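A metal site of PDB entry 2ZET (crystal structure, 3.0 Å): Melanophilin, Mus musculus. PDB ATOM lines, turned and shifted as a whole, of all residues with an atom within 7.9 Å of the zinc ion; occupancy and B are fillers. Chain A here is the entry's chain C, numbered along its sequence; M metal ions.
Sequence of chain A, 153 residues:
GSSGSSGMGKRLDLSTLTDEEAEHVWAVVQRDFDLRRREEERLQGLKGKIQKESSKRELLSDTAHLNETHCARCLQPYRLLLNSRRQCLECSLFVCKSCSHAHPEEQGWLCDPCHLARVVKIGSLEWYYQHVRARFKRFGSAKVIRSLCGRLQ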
ATOM      1  N   ARG A  57       6.847  15.528  17.158  1.00  0.00           N
ATOM      2  CA  ARG A  57       7.711  14.488  16.609  1.00  0.00           C
ATOM      3  C   ARG A  57       6.955  13.653  15.578  1.00  0.00           C
ATOM      4  O   ARG A  57       7.496  13.287  14.539  1.00  0.00           O
ATOM      5  CB  ARG A  57       8.216  13.547  17.719  1.00  0.00           C
ATOM      6  CG  ARG A  57       9.256  14.147  18.660  1.00  0.00           C
ATOM      7  CD  ARG A  57       9.792  13.076  19.612  1.00  0.00           C
ATOM      8  NE  ARG A  57      10.764  13.626  20.562  1.00  0.00           N
ATOM      9  CZ  ARG A  57      11.481  12.900  21.425  1.00  0.00           C
ATOM     10  NH1 ARG A  57      11.334  11.577  21.465  1.00  0.00           N
ATOM     11  NH2 ARG A  57      12.340  13.492  22.244  1.00  0.00           N
ATOM     12  N   ALA A  72      16.168  18.440  17.605  1.00  0.00           N
ATOM     13  CA  ALA A  72      14.877  17.754  17.681  1.00  0.00           C
ATOM     14  C   ALA A  72      13.831  18.484  18.529  1.00  0.00           C
ATOM     15  O   ALA A  72      12.633  18.241  18.389  1.00  0.00           O
ATOM     16  CB  ALA A  72      15.084  16.333  18.223  1.00  0.00           C
ATOM     17  N   GLN A  87      23.252  13.543  21.943  1.00  0.00           N
ATOM     18  CA  GLN A  87      22.284  12.474  21.702  1.00  0.00           C
ATOM     19  C   GLN A  87      21.531  12.138  22.989  1.00  0.00           C
ATOM     20  O   GLN A  87      22.136  12.057  24.059  1.00  0.00           O
ATOM     21  CB  GLN A  87      22.986  11.212  21.233  1.00  0.00           C
ATOM     22  CG  GLN A  87      22.931  10.947  19.755  1.00  0.00           C
ATOM     23  CD  GLN A  87      22.506   9.519  19.453  1.00  0.00           C
ATOM     24  OE1 GLN A  87      21.366   9.142  19.699  1.00  0.00           O
ATOM     25  NE2 GLN A  87      23.445   8.709  18.938  1.00  0.00           N
ATOM     26  N   CYS A  88      20.224  11.946  22.901  1.00  0.00           N
ATOM     27  CA  CYS A  88      19.502  11.577  24.114  1.00  0.00           C
ATOM     28  C   CYS A  88      19.796  10.117  24.361  1.00  0.00           C
ATOM     29  O   CYS A  88      19.673   9.297  23.439  1.00  0.00           O
ATOM     30  CB  CYS A  88      17.985  11.763  23.962  1.00  0.00           C
ATOM     31  SG  CYS A  88      17.066  11.443  25.515  1.00  0.00           S
ATOM     32  N   LEU A  89      20.188   9.769  25.582  1.00  0.00           N
ATOM     33  CA  LEU A  89      20.491   8.385  25.892  1.00  0.00           C
ATOM     34  C   LEU A  89      19.238   7.532  25.827  1.00  0.00           C
ATOM     35  O   LEU A  89      19.333   6.306  25.800  1.00  0.00           O
ATOM     36  CB  LEU A  89      21.134   8.254  27.262  1.00  0.00           C
ATOM     37  CG  LEU A  89      22.569   8.763  27.365  1.00  0.00           C
ATOM     38  CD1 LEU A  89      23.194   8.303  28.691  1.00  0.00           C
ATOM     39  CD2 LEU A  89      23.394   8.242  26.171  1.00  0.00           C
ATOM     40  N   GLU A  90      18.081   8.196  25.781  1.00  0.00           N
ATOM     41  CA  GLU A  90      16.797   7.515  25.762  1.00  0.00           C
ATOM     42  C   GLU A  90      16.198   7.269  24.380  1.00  0.00           C
ATOM     43  O   GLU A  90      16.083   6.116  23.956  1.00  0.00           O
ATOM     44  CB  GLU A  90      15.782   8.305  26.591  1.00  0.00           C
ATOM     45  CG  GLU A  90      14.444   7.611  26.778  1.00  0.00           C
ATOM     46  CD  GLU A  90      14.565   6.270  27.472  1.00  0.00           C
ATOM     47  OE1 GLU A  90      15.362   6.144  28.433  1.00  0.00           O
ATOM     48  OE2 GLU A  90      13.847   5.318  27.072  1.00  0.00           O
ATOM     49  N   CYS A  91      15.815   8.342  23.696  1.00  0.00           N
ATOM     50  CA  CYS A  91      15.215   8.201  22.370  1.00  0.00           C
ATOM     51  C   CYS A  91      16.247   8.395  21.248  1.00  0.00           C
ATOM     52  O   CYS A  91      15.899   8.457  20.069  1.00  0.00           O
ATOM     53  CB  CYS A  91      14.075   9.209  22.205  1.00  0.00           C
ATOM     54  SG  CYS A  91      14.622  10.873  21.870  1.00  0.00           S
ATOM     55  N   SER A  92      17.514   8.472  21.649  1.00  0.00           N
ATOM     56  CA  SER A  92      18.645   8.642  20.734  1.00  0.00           C
ATOM     57  C   SER A  92      18.542   9.633  19.576  1.00  0.00           C
ATOM     58  O   SER A  92      19.083   9.379  18.506  1.00  0.00           O
ATOM     59  CB  SER A  92      19.088   7.272  20.208  1.00  0.00           C
ATOM     60  OG  SER A  92      18.018   6.559  19.620  1.00  0.00           O
ATOM     61  N   LEU A  93      17.850  10.752  19.788  1.00  0.00           N
ATOM     62  CA  LEU A  93      17.757  11.795  18.766  1.00  0.00           C
ATOM     63  C   LEU A  93      18.720  12.868  19.237  1.00  0.00           C
ATOM     64  O   LEU A  93      19.159  12.844  20.386  1.00  0.00           O
ATOM     65  CB  LEU A  93      16.347  12.384  18.673  1.00  0.00           C
ATOM     66  CG  LEU A  93      15.240  11.508  18.084  1.00  0.00           C
ATOM     67  CD1 LEU A  93      14.013  12.368  17.764  1.00  0.00           C
ATOM     68  CD2 LEU A  93      15.736  10.826  16.813  1.00  0.00           C
ATOM     69  N   PHE A  94      19.063  13.824  18.377  1.00  0.00           N
ATOM     70  CA  PHE A  94      19.991  14.853  18.807  1.00  0.00           C
ATOM     71  C   PHE A  94      19.278  16.135  19.133  1.00  0.00           C
ATOM     72  O   PHE A  94      18.242  16.449  18.556  1.00  0.00           O
ATOM     73  CB  PHE A  94      21.039  15.124  17.741  1.00  0.00           C
ATOM     74  CG  PHE A  94      21.844  13.920  17.359  1.00  0.00           C
ATOM     75  CD1 PHE A  94      21.258  12.875  16.633  1.00  0.00           C
ATOM     76  CD2 PHE A  94      23.178  13.832  17.710  1.00  0.00           C
ATOM     77  CE1 PHE A  94      21.994  11.763  16.263  1.00  0.00           C
ATOM     78  CE2 PHE A  94      23.936  12.712  17.347  1.00  0.00           C
ATOM     79  CZ  PHE A  94      23.338  11.674  16.623  1.00  0.00           C
ATOM     80  N   VAL A  95      19.855  16.888  20.066  1.00  0.00           N
ATOM     81  CA  VAL A  95      19.304  18.153  20.492  1.00  0.00           C
ATOM     82  C   VAL A  95      20.443  19.045  20.955  1.00  0.00           C
ATOM     83  O   VAL A  95      21.537  18.560  21.265  1.00  0.00           O
ATOM     84  CB  VAL A  95      18.335  17.967  21.653  1.00  0.00           C
ATOM     85  CG1 VAL A  95      17.247  16.991  21.265  1.00  0.00           C
ATOM     86  CG2 VAL A  95      19.070  17.444  22.855  1.00  0.00           C
ATOM     87  N   TRP A 109      23.405  12.271  28.416  1.00  0.00           N
ATOM     88  CA  TRP A 109      22.365  13.304  28.523  1.00  0.00           C
ATOM     89  C   TRP A 109      20.968  12.787  28.167  1.00  0.00           C
ATOM     90  O   TRP A 109      20.789  11.633  27.764  1.00  0.00           O
ATOM     91  CB  TRP A 109      22.692  14.481  27.615  1.00  0.00           C
ATOM     92  CG  TRP A 109      24.115  14.920  27.651  1.00  0.00           C
ATOM     93  CD1 TRP A 109      25.177  14.339  27.016  1.00  0.00           C
ATOM     94  CD2 TRP A 109      24.647  16.057  28.344  1.00  0.00           C
ATOM     95  NE1 TRP A 109      26.332  15.039  27.267  1.00  0.00           N
ATOM     96  CE2 TRP A 109      26.031  16.104  28.071  1.00  0.00           C
ATOM     97  CE3 TRP A 109      24.079  17.046  29.162  1.00  0.00           C
ATOM     98  CZ2 TRP A 109      26.866  17.093  28.601  1.00  0.00           C
ATOM     99  CZ3 TRP A 109      24.905  18.037  29.683  1.00  0.00           C
ATOM    100  CH2 TRP A 109      26.284  18.050  29.400  1.00  0.00           C
ATOM    101  N   LEU A 110      19.978  13.678  28.312  1.00  0.00           N
ATOM    102  CA  LEU A 110      18.569  13.414  27.987  1.00  0.00           C
ATOM    103  C   LEU A 110      17.972  14.633  27.311  1.00  0.00           C
ATOM    104  O   LEU A 110      18.340  15.764  27.650  1.00  0.00           O
ATOM    105  CB  LEU A 110      17.768  13.117  29.256  1.00  0.00           C
ATOM    106  CG  LEU A 110      17.952  11.798  29.992  1.00  0.00           C
ATOM    107  CD1 LEU A 110      16.994  11.753  31.165  1.00  0.00           C
ATOM    108  CD2 LEU A 110      17.707  10.635  29.043  1.00  0.00           C
ATOM    109  N   CYS A 111      17.049  14.429  26.380  1.00  0.00           N
ATOM    110  CA  CYS A 111      16.409  15.551  25.692  1.00  0.00           C
ATOM    111  C   CYS A 111      15.325  16.154  26.586  1.00  0.00           C
ATOM    112  O   CYS A 111      14.645  15.418  27.300  1.00  0.00           O
ATOM    113  CB  CYS A 111      15.816  15.112  24.352  1.00  0.00           C
ATOM    114  SG  CYS A 111      14.569  13.820  24.418  1.00  0.00           S
ATOM    115  N   ASP A 112      15.163  17.475  26.554  1.00  0.00           N
ATOM    116  CA  ASP A 112      14.160  18.132  27.409  1.00  0.00           C
ATOM    117  C   ASP A 112      12.821  17.405  27.532  1.00  0.00           C
ATOM    118  O   ASP A 112      12.150  17.512  28.547  1.00  0.00           O
ATOM    119  CB  ASP A 112      13.953  19.593  26.991  1.00  0.00           C
ATOM    120  CG  ASP A 112      14.690  20.565  27.915  1.00  0.00           C
ATOM    121  OD1 ASP A 112      14.485  20.463  29.141  1.00  0.00           O
ATOM    122  OD2 ASP A 112      15.481  21.416  27.437  1.00  0.00           O
ATOM    123  N   PRO A 113      12.405  16.701  26.484  1.00  0.00           N
ATOM    124  CA  PRO A 113      11.139  15.991  26.629  1.00  0.00           C
ATOM    125  C   PRO A 113      11.350  14.753  27.491  1.00  0.00           C
ATOM    126  O   PRO A 113      10.682  14.582  28.506  1.00  0.00           O
ATOM    127  CB  PRO A 113      10.776  15.640  25.194  1.00  0.00           C
ATOM    128  CG  PRO A 113      11.309  16.788  24.459  1.00  0.00           C
ATOM    129  CD  PRO A 113      12.674  16.957  25.065  1.00  0.00           C
ATOM    130  N   CYS A 114      12.292  13.905  27.093  1.00  0.00           N
ATOM    131  CA  CYS A 114      12.586  12.683  27.839  1.00  0.00           C
ATOM    132  C   CYS A 114      12.855  12.959  29.312  1.00  0.00           C
ATOM    133  O   CYS A 114      12.578  12.117  30.168  1.00  0.00           O
ATOM    134  CB  CYS A 114      13.791  11.953  27.222  1.00  0.00           C
ATOM    135  SG  CYS A 114      13.451  11.023  25.684  1.00  0.00           S
ATOM    136  N   HIS A 115      13.386  14.142  29.612  1.00  0.00           N
ATOM    137  CA  HIS A 115      13.658  14.547  30.985  1.00  0.00           C
ATOM    138  C   HIS A 115      12.360  14.739  31.733  1.00  0.00           C
ATOM    139  O   HIS A 115      12.181  14.206  32.819  1.00  0.00           O
ATOM    140  CB  HIS A 115      14.478  15.840  31.019  1.00  0.00           C
ATOM    141  CG  HIS A 115      14.664  16.410  32.393  1.00  0.00           C
ATOM    142  ND1 HIS A 115      13.976  17.517  32.844  1.00  0.00           N
ATOM    143  CD2 HIS A 115      15.457  16.024  33.423  1.00  0.00           C
ATOM    144  CE1 HIS A 115      14.347  17.804  34.075  1.00  0.00           C
ATOM    145  NE2 HIS A 115      15.249  16.906  34.453  1.00  0.00           N
HETATM  146 ZN    ZN M   1      15.067  11.507  23.987  1.00  0.00          ZN
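N of Cys 88 lies within hydrogen-bond range of O of Leu 93 (2.9 Å). The backbone NH (N) of Glu 90 lies close to the side-chain sulfur (SG) of Cys 88 (3.4 Å). The side-chain sulfur (SG) of Cys 91 lies close to the guanidinium group (NH1) of Arg 57 (3.4 Å). The guanidinium group (NH2) of Arg 57 lies close to the side-chain sulfur (SG) of Cys 111 (3.1 Å).
The zinc ion is bound by SG of Cys 91 (2.3 Å). SG of Cys 114 binds the zinc ion (2.4 Å). SG of Cys 111 is bound to the zinc ion (2.4 Å). SG of Cys 88 binds the zinc ion, at 2.5 Å.
Residues that only touch the zinc ion: Arg 57 (3.8 Å). Of the 18 residues printed, 5 come within 4 Å of the zinc ion.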
